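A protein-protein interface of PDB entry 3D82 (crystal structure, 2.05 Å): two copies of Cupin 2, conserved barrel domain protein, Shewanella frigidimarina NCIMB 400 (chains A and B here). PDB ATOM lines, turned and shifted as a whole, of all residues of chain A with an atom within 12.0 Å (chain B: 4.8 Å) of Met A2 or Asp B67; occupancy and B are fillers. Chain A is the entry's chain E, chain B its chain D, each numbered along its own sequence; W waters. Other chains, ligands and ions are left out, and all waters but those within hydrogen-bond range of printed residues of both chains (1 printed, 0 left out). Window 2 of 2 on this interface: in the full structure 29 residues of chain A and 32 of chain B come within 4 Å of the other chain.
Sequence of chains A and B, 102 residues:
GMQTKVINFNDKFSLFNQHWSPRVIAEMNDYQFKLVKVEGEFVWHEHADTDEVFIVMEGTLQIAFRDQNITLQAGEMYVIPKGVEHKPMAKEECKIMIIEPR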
ATOM      1  N   GLY A   1      16.728 -22.054  16.144  1.00  0.00           N
ATOM      2  CA  GLY A   1      15.814 -21.493  17.182  1.00  0.00           C
ATOM      3  C   GLY A   1      14.373 -21.906  16.952  1.00  0.00           C
ATOM      4  O   GLY A   1      13.995 -22.266  15.831  1.00  0.00           O
ATOM      5  N   MET A   2      13.576 -21.851  18.025  1.00  0.00           N
ATOM      6  CA  MET A   2      12.139 -22.198  17.998  1.00  0.00           C
ATOM      7  C   MET A   2      11.302 -21.305  17.080  1.00  0.00           C
ATOM      8  O   MET A   2      10.295 -21.765  16.538  1.00  0.00           O
ATOM      9  CB  MET A   2      11.541 -22.162  19.405  1.00  0.00           C
ATOM     10  CG  MET A   2      12.046 -23.269  20.314  1.00  0.00           C
ATOM     11  SD  MET A   2      11.237 -23.123  22.090  1.00  0.00           S
ATOM     12  CE  MET A   2      12.404 -24.430  23.114  1.00  0.00           C
ATOM     13  N   GLN A   3      11.721 -20.042  16.908  1.00  0.00           N
ATOM     14  CA  GLN A   3      11.056 -19.092  16.003  1.00  0.00           C
ATOM     15  C   GLN A   3      10.894 -19.664  14.592  1.00  0.00           C
ATOM     16  O   GLN A   3       9.879 -19.407  13.949  1.00  0.00           O
ATOM     17  CB  GLN A   3      11.803 -17.741  15.946  1.00  0.00           C
ATOM     18  CG  GLN A   3      11.094 -16.628  15.126  1.00  0.00           C
ATOM     19  CD  GLN A   3       9.727 -16.224  15.701  1.00  0.00           C
ATOM     20  OE1 GLN A   3       9.598 -15.954  16.900  1.00  0.00           O
ATOM     21  NE2 GLN A   3       8.716 -16.151  14.836  1.00  0.00           N
ATOM     22  N   THR A   4      11.873 -20.465  14.139  1.00  0.00           N
ATOM     23  CA  THR A   4      11.810 -21.128  12.816  1.00  0.00           C
ATOM     24  C   THR A   4      10.576 -22.039  12.663  1.00  0.00           C
ATOM     25  O   THR A   4      10.152 -22.271  11.526  1.00  0.00           O
ATOM     26  CB  THR A   4      13.100 -21.957  12.461  1.00  0.00           C
ATOM     27  OG1 THR A   4      13.257 -23.063  13.369  1.00  0.00           O
ATOM     28  CG2 THR A   4      14.365 -21.076  12.465  1.00  0.00           C
ATOM     29  N   LYS A   5      10.029 -22.546  13.791  1.00  0.00           N
ATOM     30  CA  LYS A   5       8.814 -23.378  13.808  1.00  0.00           C
ATOM     31  C   LYS A   5       7.517 -22.578  13.984  1.00  0.00           C
ATOM     32  O   LYS A   5       6.452 -23.189  14.120  1.00  0.00           O
ATOM     33  CB  LYS A   5       8.949 -24.545  14.806  1.00  0.00           C
ATOM     34  CG  LYS A   5      10.002 -25.561  14.320  1.00  0.00           C
ATOM     35  CD  LYS A   5      10.437 -26.580  15.381  1.00  0.00           C
ATOM     36  CE  LYS A   5      11.574 -27.495  14.826  1.00  0.00           C
ATOM     37  NZ  LYS A   5      12.293 -28.328  15.872  1.00  0.00           N
ATOM     38  N   VAL A   6       7.599 -21.235  13.962  1.00  0.00           N
ATOM     39  CA  VAL A   6       6.407 -20.365  13.896  1.00  0.00           C
ATOM     40  C   VAL A   6       5.938 -20.460  12.443  1.00  0.00           C
ATOM     41  O   VAL A   6       6.715 -20.190  11.534  1.00  0.00           O
ATOM     42  CB  VAL A   6       6.683 -18.888  14.295  1.00  0.00           C
ATOM     43  CG1 VAL A   6       5.525 -17.964  13.916  1.00  0.00           C
ATOM     44  CG2 VAL A   6       6.947 -18.803  15.779  1.00  0.00           C
ATOM     45  N   ILE A   7       4.698 -20.887  12.242  1.00  0.00           N
ATOM     46  CA  ILE A   7       4.110 -21.082  10.910  1.00  0.00           C
ATOM     47  C   ILE A   7       3.223 -19.896  10.508  1.00  0.00           C
ATOM     48  O   ILE A   7       2.260 -19.595  11.212  1.00  0.00           O
ATOM     49  CB  ILE A   7       3.245 -22.374  10.840  1.00  0.00           C
ATOM     50  CG1 ILE A   7       4.058 -23.625  11.231  1.00  0.00           C
ATOM     51  CG2 ILE A   7       2.621 -22.549   9.457  1.00  0.00           C
ATOM     52  CD1 ILE A   7       3.650 -24.234  12.557  1.00  0.00           C
ATOM     53  N   ASN A   8       3.556 -19.247   9.388  1.00  0.00           N
ATOM     54  CA  ASN A   8       2.780 -18.138   8.819  1.00  0.00           C
ATOM     55  C   ASN A   8       1.958 -18.723   7.669  1.00  0.00           C
ATOM     56  O   ASN A   8       2.535 -19.206   6.680  1.00  0.00           O
ATOM     57  CB  ASN A   8       3.713 -17.008   8.350  1.00  0.00           C
ATOM     58  CG  ASN A   8       2.965 -15.833   7.741  1.00  0.00           C
ATOM     59  OD1 ASN A   8       2.430 -15.932   6.634  1.00  0.00           O
ATOM     60  ND2 ASN A   8       2.943 -14.704   8.453  1.00  0.00           N
ATOM     61  N   LYS A  12       3.117 -20.079   3.848  1.00  0.00           N
ATOM     62  CA  LYS A  12       2.910 -21.481   3.419  1.00  0.00           C
ATOM     63  C   LYS A  12       2.045 -21.614   2.170  1.00  0.00           C
ATOM     64  O   LYS A  12       2.390 -22.412   1.279  1.00  0.00           O
ATOM     65  CB  LYS A  12       2.404 -22.366   4.556  1.00  0.00           C
ATOM     66  CG  LYS A  12       3.393 -22.522   5.736  1.00  0.00           C
ATOM     67  CD  LYS A  12       4.774 -23.010   5.330  1.00  0.00           C
ATOM     68  CE  LYS A  12       5.669 -23.352   6.511  1.00  0.00           C
ATOM     69  NZ  LYS A  12       7.037 -23.662   5.977  1.00  0.00           N
ATOM     70  N   ILE A  25       1.207 -28.751   7.304  1.00  0.00           N
ATOM     71  CA  ILE A  25       2.054 -27.655   7.863  1.00  0.00           C
ATOM     72  C   ILE A  25       2.407 -27.810   9.342  1.00  0.00           C
ATOM     73  O   ILE A  25       3.321 -27.151   9.830  1.00  0.00           O
ATOM     74  CB  ILE A  25       1.436 -26.254   7.623  1.00  0.00           C
ATOM     75  CG1 ILE A  25       0.030 -26.132   8.205  1.00  0.00           C
ATOM     76  CG2 ILE A  25       1.394 -25.968   6.134  1.00  0.00           C
ATOM     77  CD1 ILE A  25      -0.452 -24.693   8.281  1.00  0.00           C
ATOM     78  N   ALA A  26       1.684 -28.673  10.050  1.00  0.00           N
ATOM     79  CA  ALA A  26       1.912 -28.873  11.462  1.00  0.00           C
ATOM     80  C   ALA A  26       1.239 -30.150  11.939  1.00  0.00           C
ATOM     81  O   ALA A  26       0.271 -30.642  11.312  1.00  0.00           O
ATOM     82  CB  ALA A  26       1.368 -27.642  12.260  1.00  0.00           C
ATOM     83  N   PHE B  65       9.877 -19.224  26.598  1.00  0.00           N
ATOM     84  CA  PHE B  65      10.353 -20.556  26.951  1.00  0.00           C
ATOM     85  C   PHE B  65      11.506 -20.329  27.900  1.00  0.00           C
ATOM     86  O   PHE B  65      11.991 -19.211  28.022  1.00  0.00           O
ATOM     87  CB  PHE B  65      10.730 -21.365  25.713  1.00  0.00           C
ATOM     88  CG  PHE B  65       9.563 -21.618  24.814  1.00  0.00           C
ATOM     89  CD1 PHE B  65       9.253 -20.731  23.783  1.00  0.00           C
ATOM     90  CD2 PHE B  65       8.714 -22.700  25.045  1.00  0.00           C
ATOM     91  CE1 PHE B  65       8.134 -20.943  22.963  1.00  0.00           C
ATOM     92  CE2 PHE B  65       7.575 -22.911  24.241  1.00  0.00           C
ATOM     93  CZ  PHE B  65       7.289 -22.029  23.199  1.00  0.00           C
ATOM     94  N   ARG B  66      11.950 -21.379  28.578  1.00  0.00           N
ATOM     95  CA  ARG B  66      13.051 -21.251  29.541  1.00  0.00           C
ATOM     96  C   ARG B  66      14.417 -20.859  28.972  1.00  0.00           C
ATOM     97  O   ARG B  66      15.256 -20.344  29.710  1.00  0.00           O
ATOM     98  CB  ARG B  66      13.185 -22.526  30.368  1.00  0.00           C
ATOM     99  CG  ARG B  66      12.000 -22.802  31.261  1.00  0.00           C
ATOM    100  CD  ARG B  66      11.808 -21.696  32.294  1.00  0.00           C
ATOM    101  NE  ARG B  66      10.858 -22.081  33.304  1.00  0.00           N
ATOM    102  CZ  ARG B  66      10.501 -21.320  34.337  1.00  0.00           C
ATOM    103  NH1 ARG B  66      10.979 -20.080  34.508  1.00  0.00           N
ATOM    104  NH2 ARG B  66       9.632 -21.813  35.202  1.00  0.00           N
ATOM    105  N   ASP B  67      14.618 -21.107  27.681  1.00  0.00           N
ATOM    106  CA  ASP B  67      15.868 -20.814  26.977  1.00  0.00           C
ATOM    107  C   ASP B  67      15.760 -19.713  25.909  1.00  0.00           C
ATOM    108  O   ASP B  67      16.782 -19.170  25.507  1.00  0.00           O
ATOM    109  CB  ASP B  67      16.430 -22.108  26.349  1.00  0.00           C
ATOM    110  CG  ASP B  67      15.459 -22.792  25.363  1.00  0.00           C
ATOM    111  OD1 ASP B  67      14.214 -22.671  25.512  1.00  0.00           O
ATOM    112  OD2 ASP B  67      15.953 -23.505  24.462  1.00  0.00           O
ATOM    113  N   GLN B  68      14.545 -19.364  25.487  1.00  0.00           N
ATOM    114  CA  GLN B  68      14.317 -18.400  24.400  1.00  0.00           C
ATOM    115  C   GLN B  68      12.855 -17.944  24.340  1.00  0.00           C
ATOM    116  O   GLN B  68      12.016 -18.431  25.099  1.00  0.00           O
ATOM    117  CB  GLN B  68      14.691 -19.061  23.064  1.00  0.00           C
ATOM    118  CG  GLN B  68      13.912 -20.358  22.756  1.00  0.00           C
ATOM    119  CD  GLN B  68      14.460 -21.083  21.546  1.00  0.00           C
ATOM    120  OE1 GLN B  68      14.292 -20.628  20.403  1.00  0.00           O
ATOM    121  NE2 GLN B  68      15.094 -22.238  21.781  1.00  0.00           N
ATOM    122  N   ILE B  70       9.581 -16.668  21.464  1.00  0.00           N
ATOM    123  CA  ILE B  70       9.034 -16.581  20.114  1.00  0.00           C
ATOM    124  C   ILE B  70       7.942 -15.504  20.114  1.00  0.00           C
ATOM    125  O   ILE B  70       7.423 -15.158  21.168  1.00  0.00           O
ATOM    126  CB  ILE B  70       8.511 -17.940  19.571  1.00  0.00           C
ATOM    127  CG1 ILE B  70       7.214 -18.383  20.257  1.00  0.00           C
ATOM    128  CG2 ILE B  70       9.631 -19.010  19.648  1.00  0.00           C
ATOM    129  CD1 ILE B  70       6.678 -19.697  19.744  1.00  0.00           C
ATOM    130  N   TYR B  78       1.730 -21.869  16.288  1.00  0.00           N
ATOM    131  CA  TYR B  78       2.838 -22.605  16.901  1.00  0.00           C
ATOM    132  C   TYR B  78       2.282 -23.779  17.697  1.00  0.00           C
ATOM    133  O   TYR B  78       1.264 -23.627  18.357  1.00  0.00           O
ATOM    134  CB  TYR B  78       3.645 -21.673  17.824  1.00  0.00           C
ATOM    135  CG  TYR B  78       4.962 -22.251  18.249  1.00  0.00           C
ATOM    136  CD1 TYR B  78       6.099 -22.112  17.443  1.00  0.00           C
ATOM    137  CD2 TYR B  78       5.079 -22.983  19.431  1.00  0.00           C
ATOM    138  CE1 TYR B  78       7.340 -22.669  17.834  1.00  0.00           C
ATOM    139  CE2 TYR B  78       6.313 -23.553  19.832  1.00  0.00           C
ATOM    140  CZ  TYR B  78       7.439 -23.396  19.039  1.00  0.00           C
ATOM    141  OH  TYR B  78       8.640 -23.952  19.451  1.00  0.00           O
HETATM  142  O   HOH W   1       9.017 -25.390  21.920  1.00  0.00           O
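Met A2 touches five residues of chain B. Asp B67 touches one residue of chain A. Of chain A, only Gly A1 (3.7 Å) and Met A2 (2.8 Å) come within 4 Å of Gln B68. Of the printed residues of chain B, Val A6 touches Tyr B78 (3.8 Å). Printed residues of chain B within 4 Å of Gly A1: Gln B68 (3.7 Å). Of the printed residues of chain B, Lys A5 touches Tyr B78. Of the printed residues of chain B, Gln A3 touches Ile B70. Ile A25 touches none of the printed residues of chain B.
Water W1 lies within hydrogen-bond range of the side-chain hydroxyl of Tyr B78 (2.9 Å) and the side-chain sulfur of Met A2 (3.2 Å).
Among the printed residues, pairs that only touch across the chains: Gly A1 with Gln B68 (3.7 Å), Met A2 with Phe B65 (3.5 Å), Met A2 with Asp B67 (3.5 Å), Met A2 with Ile B70 (3.7 Å), Gln A3 with Ile B70 (3.3 Å), Lys A5 with Tyr B78 (3.5 Å) and Val A6 with Tyr B78 (3.8 Å).
The side-chain amide nitrogen of Gln B68 lies within hydrogen-bond range of the side-chain carboxylate of Asp B67 (3.1 Å). O of Gly A1 lies within hydrogen-bond range of OG1 of Thr A4, 2.7 Å away.
Hydrophobic or aromatic side chains of chain A within 4 Å of the printed part of chain B: Met A2 and Val A6. Among the printed residues, no Asp or Glu carboxylate lies within 4 Å of a Lys or Arg side-chain nitrogen of the other chain.
No position is printed for both chains. Of the 9 pairs that touch across the chains among the printed residues, none has its exchanged pair printed and touching as well.
The backbone NH (N) of Met A2 sits at hydrogen-bond distance from the side-chain amide oxygen (OE1) of Gln B68 (2.8 Å). The side-chain sulfur (SD) of Met A2 lies close to the side-chain hydroxyl (OH) of Tyr B78, at 3.8 Å.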
